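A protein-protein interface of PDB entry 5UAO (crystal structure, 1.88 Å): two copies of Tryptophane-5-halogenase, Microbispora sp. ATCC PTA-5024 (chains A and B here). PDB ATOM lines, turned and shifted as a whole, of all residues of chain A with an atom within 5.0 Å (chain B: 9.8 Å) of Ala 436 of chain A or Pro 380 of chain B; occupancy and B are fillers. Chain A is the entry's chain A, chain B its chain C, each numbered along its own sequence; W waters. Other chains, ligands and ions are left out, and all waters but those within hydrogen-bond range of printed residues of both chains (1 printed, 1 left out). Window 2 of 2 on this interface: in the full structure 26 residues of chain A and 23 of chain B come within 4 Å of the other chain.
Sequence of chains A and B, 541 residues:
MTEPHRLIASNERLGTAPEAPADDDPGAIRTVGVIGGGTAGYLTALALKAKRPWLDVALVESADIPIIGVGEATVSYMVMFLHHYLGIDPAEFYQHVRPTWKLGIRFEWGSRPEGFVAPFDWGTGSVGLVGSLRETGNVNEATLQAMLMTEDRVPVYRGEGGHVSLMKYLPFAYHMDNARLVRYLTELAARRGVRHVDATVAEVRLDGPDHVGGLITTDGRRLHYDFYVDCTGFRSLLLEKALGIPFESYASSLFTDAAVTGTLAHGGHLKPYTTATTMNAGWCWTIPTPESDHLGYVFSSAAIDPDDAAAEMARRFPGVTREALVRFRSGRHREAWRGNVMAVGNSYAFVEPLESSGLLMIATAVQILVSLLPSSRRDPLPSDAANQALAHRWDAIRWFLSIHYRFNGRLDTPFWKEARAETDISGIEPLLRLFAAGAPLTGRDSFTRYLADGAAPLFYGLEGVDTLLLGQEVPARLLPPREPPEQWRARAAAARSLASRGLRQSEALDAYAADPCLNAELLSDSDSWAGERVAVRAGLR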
ATOM      1  N   LEU A 432     -16.558  -1.935  21.054  1.00  0.00           N
ATOM      2  CA  LEU A 432     -17.276  -2.504  22.241  1.00  0.00           C
ATOM      3  C   LEU A 432     -16.859  -3.943  22.572  1.00  0.00           C
ATOM      4  O   LEU A 432     -16.781  -4.321  23.767  1.00  0.00           O
ATOM      5  CB  LEU A 432     -18.782  -2.478  22.087  1.00  0.00           C
ATOM      6  CG  LEU A 432     -19.380  -1.065  21.933  1.00  0.00           C
ATOM      7  CD1 LEU A 432     -20.872  -1.110  21.655  1.00  0.00           C
ATOM      8  CD2 LEU A 432     -19.099  -0.150  23.113  1.00  0.00           C
ATOM      9  N   ARG A 433     -16.551  -4.711  21.529  1.00  0.00           N
ATOM     10  CA  ARG A 433     -16.080  -6.107  21.681  1.00  0.00           C
ATOM     11  C   ARG A 433     -14.724  -6.147  22.281  1.00  0.00           C
ATOM     12  O   ARG A 433     -14.422  -7.068  23.093  1.00  0.00           O
ATOM     13  CB  ARG A 433     -16.088  -6.870  20.360  1.00  0.00           C
ATOM     14  CG  ARG A 433     -17.478  -7.041  19.783  1.00  0.00           C
ATOM     15  CD  ARG A 433     -17.638  -8.280  18.921  1.00  0.00           C
ATOM     16  NE  ARG A 433     -18.765  -8.177  17.991  1.00  0.00           N
ATOM     17  CZ  ARG A 433     -18.754  -7.515  16.816  1.00  0.00           C
ATOM     18  NH1 ARG A 433     -17.667  -6.852  16.377  1.00  0.00           N
ATOM     19  NH2 ARG A 433     -19.859  -7.499  16.063  1.00  0.00           N
ATOM     20  N   LEU A 434     -13.879  -5.162  21.950  1.00  0.00           N
ATOM     21  CA  LEU A 434     -12.573  -5.028  22.589  1.00  0.00           C
ATOM     22  C   LEU A 434     -12.703  -4.705  24.091  1.00  0.00           C
ATOM     23  O   LEU A 434     -12.075  -5.353  24.975  1.00  0.00           O
ATOM     24  CB  LEU A 434     -11.784  -3.930  21.934  1.00  0.00           C
ATOM     25  CG  LEU A 434     -11.181  -4.113  20.523  1.00  0.00           C
ATOM     26  CD1 LEU A 434     -10.269  -2.924  20.155  1.00  0.00           C
ATOM     27  CD2 LEU A 434     -10.393  -5.408  20.382  1.00  0.00           C
ATOM     28  N   PHE A 435     -13.520  -3.686  24.365  1.00  0.00           N
ATOM     29  CA  PHE A 435     -13.847  -3.279  25.742  1.00  0.00           C
ATOM     30  C   PHE A 435     -14.260  -4.439  26.649  1.00  0.00           C
ATOM     31  O   PHE A 435     -13.736  -4.600  27.748  1.00  0.00           O
ATOM     32  CB  PHE A 435     -14.993  -2.287  25.720  1.00  0.00           C
ATOM     33  CG  PHE A 435     -15.452  -1.851  27.093  1.00  0.00           C
ATOM     34  CD1 PHE A 435     -14.827  -0.798  27.736  1.00  0.00           C
ATOM     35  CD2 PHE A 435     -16.531  -2.447  27.700  1.00  0.00           C
ATOM     36  CE1 PHE A 435     -15.278  -0.347  28.937  1.00  0.00           C
ATOM     37  CE2 PHE A 435     -16.956  -1.999  28.923  1.00  0.00           C
ATOM     38  CZ  PHE A 435     -16.307  -0.962  29.541  1.00  0.00           C
ATOM     39  N   ALA A 436     -15.212  -5.225  26.177  1.00  0.00           N
ATOM     40  CA  ALA A 436     -15.766  -6.340  26.933  1.00  0.00           C
ATOM     41  C   ALA A 436     -14.707  -7.334  27.393  1.00  0.00           C
ATOM     42  O   ALA A 436     -14.778  -7.883  28.523  1.00  0.00           O
ATOM     43  CB  ALA A 436     -16.815  -7.053  26.108  1.00  0.00           C
ATOM     44  N   ALA A 437     -13.730  -7.554  26.534  1.00  0.00           N
ATOM     45  CA  ALA A 437     -12.723  -8.568  26.772  1.00  0.00           C
ATOM     46  C   ALA A 437     -11.724  -8.058  27.788  1.00  0.00           C
ATOM     47  O   ALA A 437     -10.932  -8.835  28.330  1.00  0.00           O
ATOM     48  CB  ALA A 437     -12.016  -8.925  25.445  1.00  0.00           C
ATOM     49  N   GLY A 438     -11.712  -6.756  28.041  1.00  0.00           N
ATOM     50  CA  GLY A 438     -10.794  -6.188  29.050  1.00  0.00           C
ATOM     51  C   GLY A 438     -10.880  -4.689  29.156  1.00  0.00           C
ATOM     52  O   GLY A 438     -10.257  -3.946  28.369  1.00  0.00           O
ATOM     53  N   PRO A 475     -21.265  -4.731  30.991  1.00  0.00           N
ATOM     54  CA  PRO A 475     -20.455  -5.859  31.484  1.00  0.00           C
ATOM     55  C   PRO A 475     -19.123  -5.961  30.763  1.00  0.00           C
ATOM     56  O   PRO A 475     -19.074  -5.808  29.530  1.00  0.00           O
ATOM     57  CB  PRO A 475     -21.309  -7.093  31.153  1.00  0.00           C
ATOM     58  CG  PRO A 475     -22.673  -6.591  30.903  1.00  0.00           C
ATOM     59  CD  PRO A 475     -22.527  -5.181  30.386  1.00  0.00           C
ATOM     60  N   ALA A 476     -18.053  -6.197  31.510  1.00  0.00           N
ATOM     61  CA  ALA A 476     -16.747  -6.416  30.931  1.00  0.00           C
ATOM     62  C   ALA A 476     -15.859  -7.048  31.944  1.00  0.00           C
ATOM     63  O   ALA A 476     -16.189  -6.995  33.108  1.00  0.00           O
ATOM     64  CB  ALA A 476     -16.141  -5.110  30.456  1.00  0.00           C
ATOM     65  N   ARG A 477     -14.786  -7.712  31.486  1.00  0.00           N
ATOM     66  CA  ARG A 477     -13.735  -8.187  32.351  1.00  0.00           C
ATOM     67  C   ARG A 477     -12.921  -6.988  32.729  1.00  0.00           C
ATOM     68  O   ARG A 477     -12.338  -6.332  31.869  1.00  0.00           O
ATOM     69  CB  ARG A 477     -12.823  -9.201  31.676  1.00  0.00           C
ATOM     70  CG  ARG A 477     -13.494 -10.520  31.339  1.00  0.00           C
ATOM     71  CD  ARG A 477     -12.701 -11.693  31.918  1.00  0.00           C
ATOM     72  NE  ARG A 477     -12.746 -12.882  31.064  1.00  0.00           N
ATOM     73  CZ  ARG A 477     -11.760 -13.297  30.261  1.00  0.00           C
ATOM     74  NH1 ARG A 477     -10.610 -12.632  30.167  1.00  0.00           N
ATOM     75  NH2 ARG A 477     -11.923 -14.401  29.538  1.00  0.00           N
ATOM     76  N   ILE B  29      -8.450 -21.099  24.913  1.00  0.00           N
ATOM     77  CA  ILE B  29      -7.612 -21.308  23.745  1.00  0.00           C
ATOM     78  C   ILE B  29      -6.263 -21.677  24.338  1.00  0.00           C
ATOM     79  O   ILE B  29      -5.673 -20.853  24.971  1.00  0.00           O
ATOM     80  CB  ILE B  29      -7.560 -20.045  22.833  1.00  0.00           C
ATOM     81  CG1 ILE B  29      -8.939 -19.823  22.205  1.00  0.00           C
ATOM     82  CG2 ILE B  29      -6.480 -20.189  21.790  1.00  0.00           C
ATOM     83  CD1 ILE B  29      -9.049 -18.597  21.315  1.00  0.00           C
ATOM     84  N   TRP B 337      -9.243 -12.086   9.463  1.00  0.00           N
ATOM     85  CA  TRP B 337      -9.592 -12.916  10.660  1.00  0.00           C
ATOM     86  C   TRP B 337     -11.064 -13.289  10.509  1.00  0.00           C
ATOM     87  O   TRP B 337     -11.987 -12.445  10.421  1.00  0.00           O
ATOM     88  CB  TRP B 337      -9.222 -12.160  11.953  1.00  0.00           C
ATOM     89  CG  TRP B 337      -9.458 -12.910  13.278  1.00  0.00           C
ATOM     90  CD1 TRP B 337     -10.245 -14.034  13.499  1.00  0.00           C
ATOM     91  CD2 TRP B 337      -8.930 -12.559  14.548  1.00  0.00           C
ATOM     92  NE1 TRP B 337     -10.199 -14.397  14.821  1.00  0.00           N
ATOM     93  CE2 TRP B 337      -9.395 -13.517  15.486  1.00  0.00           C
ATOM     94  CE3 TRP B 337      -8.081 -11.560  14.988  1.00  0.00           C
ATOM     95  CZ2 TRP B 337      -9.051 -13.468  16.818  1.00  0.00           C
ATOM     96  CZ3 TRP B 337      -7.774 -11.494  16.306  1.00  0.00           C
ATOM     97  CH2 TRP B 337      -8.233 -12.450  17.213  1.00  0.00           C
ATOM     98  N   GLY B 339     -13.519 -16.237  12.399  1.00  0.00           N
ATOM     99  CA  GLY B 339     -13.699 -17.406  13.263  1.00  0.00           C
ATOM    100  C   GLY B 339     -12.415 -17.747  13.999  1.00  0.00           C
ATOM    101  O   GLY B 339     -11.775 -16.904  14.645  1.00  0.00           O
ATOM    102  N   SER B 371      -2.009  -9.440  20.544  1.00  0.00           N
ATOM    103  CA  SER B 371      -2.800  -8.549  21.410  1.00  0.00           C
ATOM    104  C   SER B 371      -4.267  -8.922  21.600  1.00  0.00           C
ATOM    105  O   SER B 371      -4.785  -8.790  22.698  1.00  0.00           O
ATOM    106  CB  SER B 371      -2.753  -7.101  20.880  1.00  0.00           C
ATOM    107  OG  SER B 371      -1.502  -6.505  21.204  1.00  0.00           O
ATOM    108  N   LEU B 372      -4.927  -9.346  20.515  1.00  0.00           N
ATOM    109  CA  LEU B 372      -6.346  -9.549  20.447  1.00  0.00           C
ATOM    110  C   LEU B 372      -6.863 -11.001  20.616  1.00  0.00           C
ATOM    111  O   LEU B 372      -8.054 -11.247  20.842  1.00  0.00           O
ATOM    112  CB  LEU B 372      -6.815  -9.000  19.119  1.00  0.00           C
ATOM    113  CG  LEU B 372      -7.042  -7.493  19.144  1.00  0.00           C
ATOM    114  CD1 LEU B 372      -5.781  -6.721  19.401  1.00  0.00           C
ATOM    115  CD2 LEU B 372      -7.684  -7.079  17.844  1.00  0.00           C
ATOM    116  N   LEU B 373      -5.977 -11.966  20.505  1.00  0.00           N
ATOM    117  CA  LEU B 373      -6.372 -13.356  20.628  1.00  0.00           C
ATOM    118  C   LEU B 373      -7.060 -13.568  21.979  1.00  0.00           C
ATOM    119  O   LEU B 373      -6.504 -13.215  23.053  1.00  0.00           O
ATOM    120  CB  LEU B 373      -5.158 -14.250  20.524  1.00  0.00           C
ATOM    121  CG  LEU B 373      -5.376 -15.767  20.640  1.00  0.00           C
ATOM    122  CD1 LEU B 373      -6.127 -16.333  19.440  1.00  0.00           C
ATOM    123  CD2 LEU B 373      -4.038 -16.441  20.825  1.00  0.00           C
ATOM    124  N   PRO B 374      -8.254 -14.134  21.923  1.00  0.00           N
ATOM    125  CA  PRO B 374      -9.025 -14.321  23.118  1.00  0.00           C
ATOM    126  C   PRO B 374      -8.407 -15.356  24.056  1.00  0.00           C
ATOM    127  O   PRO B 374      -7.634 -16.235  23.639  1.00  0.00           O
ATOM    128  CB  PRO B 374     -10.383 -14.811  22.601  1.00  0.00           C
ATOM    129  CG  PRO B 374     -10.457 -14.372  21.171  1.00  0.00           C
ATOM    130  CD  PRO B 374      -9.027 -14.481  20.711  1.00  0.00           C
ATOM    131  N   SER B 375      -8.757 -15.238  25.334  1.00  0.00           N
ATOM    132  CA  SER B 375      -8.389 -16.261  26.322  1.00  0.00           C
ATOM    133  C   SER B 375      -9.167 -17.536  26.157  1.00  0.00           C
ATOM    134  O   SER B 375      -8.624 -18.616  26.322  1.00  0.00           O
ATOM    135  CB  SER B 375      -8.565 -15.721  27.743  1.00  0.00           C
ATOM    136  OG  SER B 375      -7.405 -14.985  28.022  1.00  0.00           O
ATOM    137  N   SER B 376     -10.427 -17.418  25.792  1.00  0.00           N
ATOM    138  CA  SER B 376     -11.237 -18.575  25.605  1.00  0.00           C
ATOM    139  C   SER B 376     -12.132 -18.528  24.369  1.00  0.00           C
ATOM    140  O   SER B 376     -12.445 -17.455  23.834  1.00  0.00           O
ATOM    141  CB  SER B 376     -12.066 -18.801  26.879  1.00  0.00           C
ATOM    142  OG  SER B 376     -13.115 -17.880  26.972  1.00  0.00           O
ATOM    143  N   ARG B 377     -12.555 -19.717  23.940  1.00  0.00           N
ATOM    144  CA  ARG B 377     -13.505 -19.873  22.858  1.00  0.00           C
ATOM    145  C   ARG B 377     -14.863 -19.208  23.093  1.00  0.00           C
ATOM    146  O   ARG B 377     -15.588 -18.937  22.142  1.00  0.00           O
ATOM    147  CB  ARG B 377     -13.714 -21.356  22.529  1.00  0.00           C
ATOM    148  CG  ARG B 377     -12.907 -21.807  21.320  1.00  0.00           C
ATOM    149  CD  ARG B 377     -12.605 -23.299  21.309  1.00  0.00           C
ATOM    150  NE  ARG B 377     -11.711 -23.657  22.409  1.00  0.00           N
ATOM    151  CZ  ARG B 377     -11.708 -24.838  23.017  1.00  0.00           C
ATOM    152  NH1 ARG B 377     -12.542 -25.801  22.634  1.00  0.00           N
ATOM    153  NH2 ARG B 377     -10.871 -25.065  24.018  1.00  0.00           N
ATOM    154  N   ARG B 378     -15.231 -18.929  24.330  1.00  0.00           N
ATOM    155  CA  ARG B 378     -16.543 -18.317  24.552  1.00  0.00           C
ATOM    156  C   ARG B 378     -16.509 -16.800  24.514  1.00  0.00           C
ATOM    157  O   ARG B 378     -17.551 -16.149  24.571  1.00  0.00           O
ATOM    158  CB  ARG B 378     -17.180 -18.822  25.865  1.00  0.00           C
ATOM    159  CG  ARG B 378     -16.456 -18.475  27.164  1.00  0.00           C
ATOM    160  CD  ARG B 378     -16.758 -19.509  28.268  1.00  0.00           C
ATOM    161  NE  ARG B 378     -18.176 -19.546  28.732  1.00  0.00           N
ATOM    162  CZ  ARG B 378     -19.037 -20.582  28.627  1.00  0.00           C
ATOM    163  NH1 ARG B 378     -18.693 -21.737  28.057  1.00  0.00           N
ATOM    164  NH2 ARG B 378     -20.275 -20.468  29.112  1.00  0.00           N
ATOM    165  N   ASP B 379     -15.327 -16.217  24.399  1.00  0.00           N
ATOM    166  CA  ASP B 379     -15.195 -14.772  24.588  1.00  0.00           C
ATOM    167  C   ASP B 379     -15.671 -13.946  23.380  1.00  0.00           C
ATOM    168  O   ASP B 379     -15.979 -14.530  22.321  1.00  0.00           O
ATOM    169  CB  ASP B 379     -13.766 -14.457  24.986  1.00  0.00           C
ATOM    170  CG  ASP B 379     -13.434 -15.009  26.349  1.00  0.00           C
ATOM    171  OD1 ASP B 379     -14.382 -15.517  27.005  1.00  0.00           O
ATOM    172  OD2 ASP B 379     -12.255 -14.950  26.766  1.00  0.00           O
ATOM    173  N   PRO B 380     -15.808 -12.597  23.560  1.00  0.00           N
ATOM    174  CA  PRO B 380     -16.144 -11.797  22.389  1.00  0.00           C
ATOM    175  C   PRO B 380     -14.902 -11.718  21.468  1.00  0.00           C
ATOM    176  O   PRO B 380     -13.803 -11.287  21.882  1.00  0.00           O
ATOM    177  CB  PRO B 380     -16.576 -10.436  22.984  1.00  0.00           C
ATOM    178  CG  PRO B 380     -15.826 -10.322  24.264  1.00  0.00           C
ATOM    179  CD  PRO B 380     -15.734 -11.751  24.782  1.00  0.00           C
ATOM    180  N   LEU B 381     -15.117 -12.214  20.257  1.00  0.00           N
ATOM    181  CA  LEU B 381     -14.112 -12.268  19.202  1.00  0.00           C
ATOM    182  C   LEU B 381     -13.870 -10.895  18.549  1.00  0.00           C
ATOM    183  O   LEU B 381     -14.782 -10.337  17.962  1.00  0.00           O
ATOM    184  CB  LEU B 381     -14.615 -13.237  18.149  1.00  0.00           C
ATOM    185  CG  LEU B 381     -13.580 -13.811  17.194  1.00  0.00           C
ATOM    186  CD1 LEU B 381     -12.510 -14.667  17.883  1.00  0.00           C
ATOM    187  CD2 LEU B 381     -14.325 -14.607  16.143  1.00  0.00           C
ATOM    188  N   PRO B 382     -12.633 -10.374  18.603  1.00  0.00           N
ATOM    189  CA  PRO B 382     -12.423  -9.058  18.043  1.00  0.00           C
ATOM    190  C   PRO B 382     -11.968  -9.075  16.570  1.00  0.00           C
ATOM    191  O   PRO B 382     -11.191  -8.248  16.164  1.00  0.00           O
ATOM    192  CB  PRO B 382     -11.317  -8.506  18.935  1.00  0.00           C
ATOM    193  CG  PRO B 382     -10.478  -9.691  19.145  1.00  0.00           C
ATOM    194  CD  PRO B 382     -11.404 -10.880  19.236  1.00  0.00           C
ATOM    195  N   SER B 383     -12.528  -9.928  15.758  1.00  0.00           N
ATOM    196  CA  SER B 383     -12.114 -10.046  14.399  1.00  0.00           C
ATOM    197  C   SER B 383     -12.468  -8.820  13.578  1.00  0.00           C
ATOM    198  O   SER B 383     -11.686  -8.454  12.677  1.00  0.00           O
ATOM    199  CB  SER B 383     -12.643 -11.292  13.764  1.00  0.00           C
ATOM    200  OG  SER B 383     -13.966 -11.530  14.079  1.00  0.00           O
ATOM    201  N   ASP B 384     -13.587  -8.142  13.881  1.00  0.00           N
ATOM    202  CA  ASP B 384     -13.955  -6.970  13.087  1.00  0.00           C
ATOM    203  C   ASP B 384     -12.931  -5.882  13.255  1.00  0.00           C
ATOM    204  O   ASP B 384     -12.525  -5.237  12.280  1.00  0.00           O
ATOM    205  CB  ASP B 384     -15.336  -6.429  13.512  1.00  0.00           C
ATOM    206  CG  ASP B 384     -16.505  -7.236  12.898  1.00  0.00           C
ATOM    207  OD1 ASP B 384     -16.379  -7.894  11.821  1.00  0.00           O
ATOM    208  OD2 ASP B 384     -17.594  -7.146  13.463  1.00  0.00           O
ATOM    209  N   ALA B 385     -12.455  -5.688  14.478  1.00  0.00           N
ATOM    210  CA  ALA B 385     -11.473  -4.642  14.671  1.00  0.00           C
ATOM    211  C   ALA B 385     -10.167  -4.925  13.945  1.00  0.00           C
ATOM    212  O   ALA B 385      -9.465  -4.001  13.439  1.00  0.00           O
ATOM    213  CB  ALA B 385     -11.188  -4.454  16.132  1.00  0.00           C
HETATM  214  O   HOH W   1     -12.721  -8.634  21.780  1.00  0.00           O
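Among the printed residues, merely in contact across the chains: Leu 434 of chain A with Pro 382 of chain B (3.5 Å), Arg 433 of chain A with Leu 381 of chain B (3.6 Å), Arg 433 of chain A with Pro 380 of chain B (3.7 Å) and Ala 436 of chain A with Pro 380 of chain B (3.9 Å).
Printed residues of chain B within 4 Å of Arg 433 of chain A: Pro 380, Leu 381 and Asp 384.
Printed residues of chain B within 4 Å of Leu 434 of chain A: Pro 382 (3.5 Å).
No residue of chain B comes within 4 Å of Phe 435 of chain A.
No residue of chain B comes within 4 Å of Ala 437 of chain A.
Pro 475 of chain A touches none of the printed residues of chain B.
No residue of chain B comes within 4 Å of Ala 476 of chain A.
Printed residues of chain A within 4 Å of Asp 379 of chain B: Arg 477.
Of the printed residues of chain A, Leu 381 of chain B touches Arg 433.
Of the printed residues of chain A, Asp 384 of chain B touches Arg 433.
The nearest residue of chain B that does not touch Ala 436 of chain A is Asp 379 of chain B (7.5 Å).
The nearest residue of chain A that does not touch Pro 380 of chain B is Ala 437 of chain A (4.1 Å).
The nearest printed residue of chain A that does not touch Asp 384 of chain B is Leu 434 of chain A (7.6 Å).
Water W1 lies within hydrogen-bond range of O of Arg 433 of chain A (2.7 Å) and O of Pro 380 of chain B (2.9 Å).
Hydrophobic or aromatic side chains of chain A that line the printed part of chain B: Leu 434 and Ala 436.
Along chain B the printed residues that touch a printed residue of chain A span positions 379 to 384.
Among the printed residues, Asp or Glu carboxylates within 4 Å of a Lys or Arg side-chain nitrogen of the other chain: Arg 433 of chain A with Asp 384 of chain B (2.9 Å) and Arg 477 of chain A with Asp 379 of chain B (2.8 Å).
The guanidinium group (NH1) of Arg 433 of chain A lies within salt-bridge range of the side-chain carboxylate (OD2) of Asp 384 of chain B (2.9 Å).
The guanidinium group (NH2) of Arg 477 of chain A is in salt-bridge range of the side-chain carboxylate (OD2) of Asp 379 of chain B (2.8 Å).
The backbone NH (N) of Arg 477 of chain A lies within hydrogen-bond range of the backbone carbonyl oxygen (O) of Ala 436 of chain A (3.0 Å).
The side-chain carboxylate of Asp 379 of chain B sits at hydrogen-bond distance from the side-chain hydroxyl of Ser 376 of chain B.
No position is printed for both chains.
Of the 6 pairs that touch across the chains among the printed residues, none has its exchanged pair printed and touching as well.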
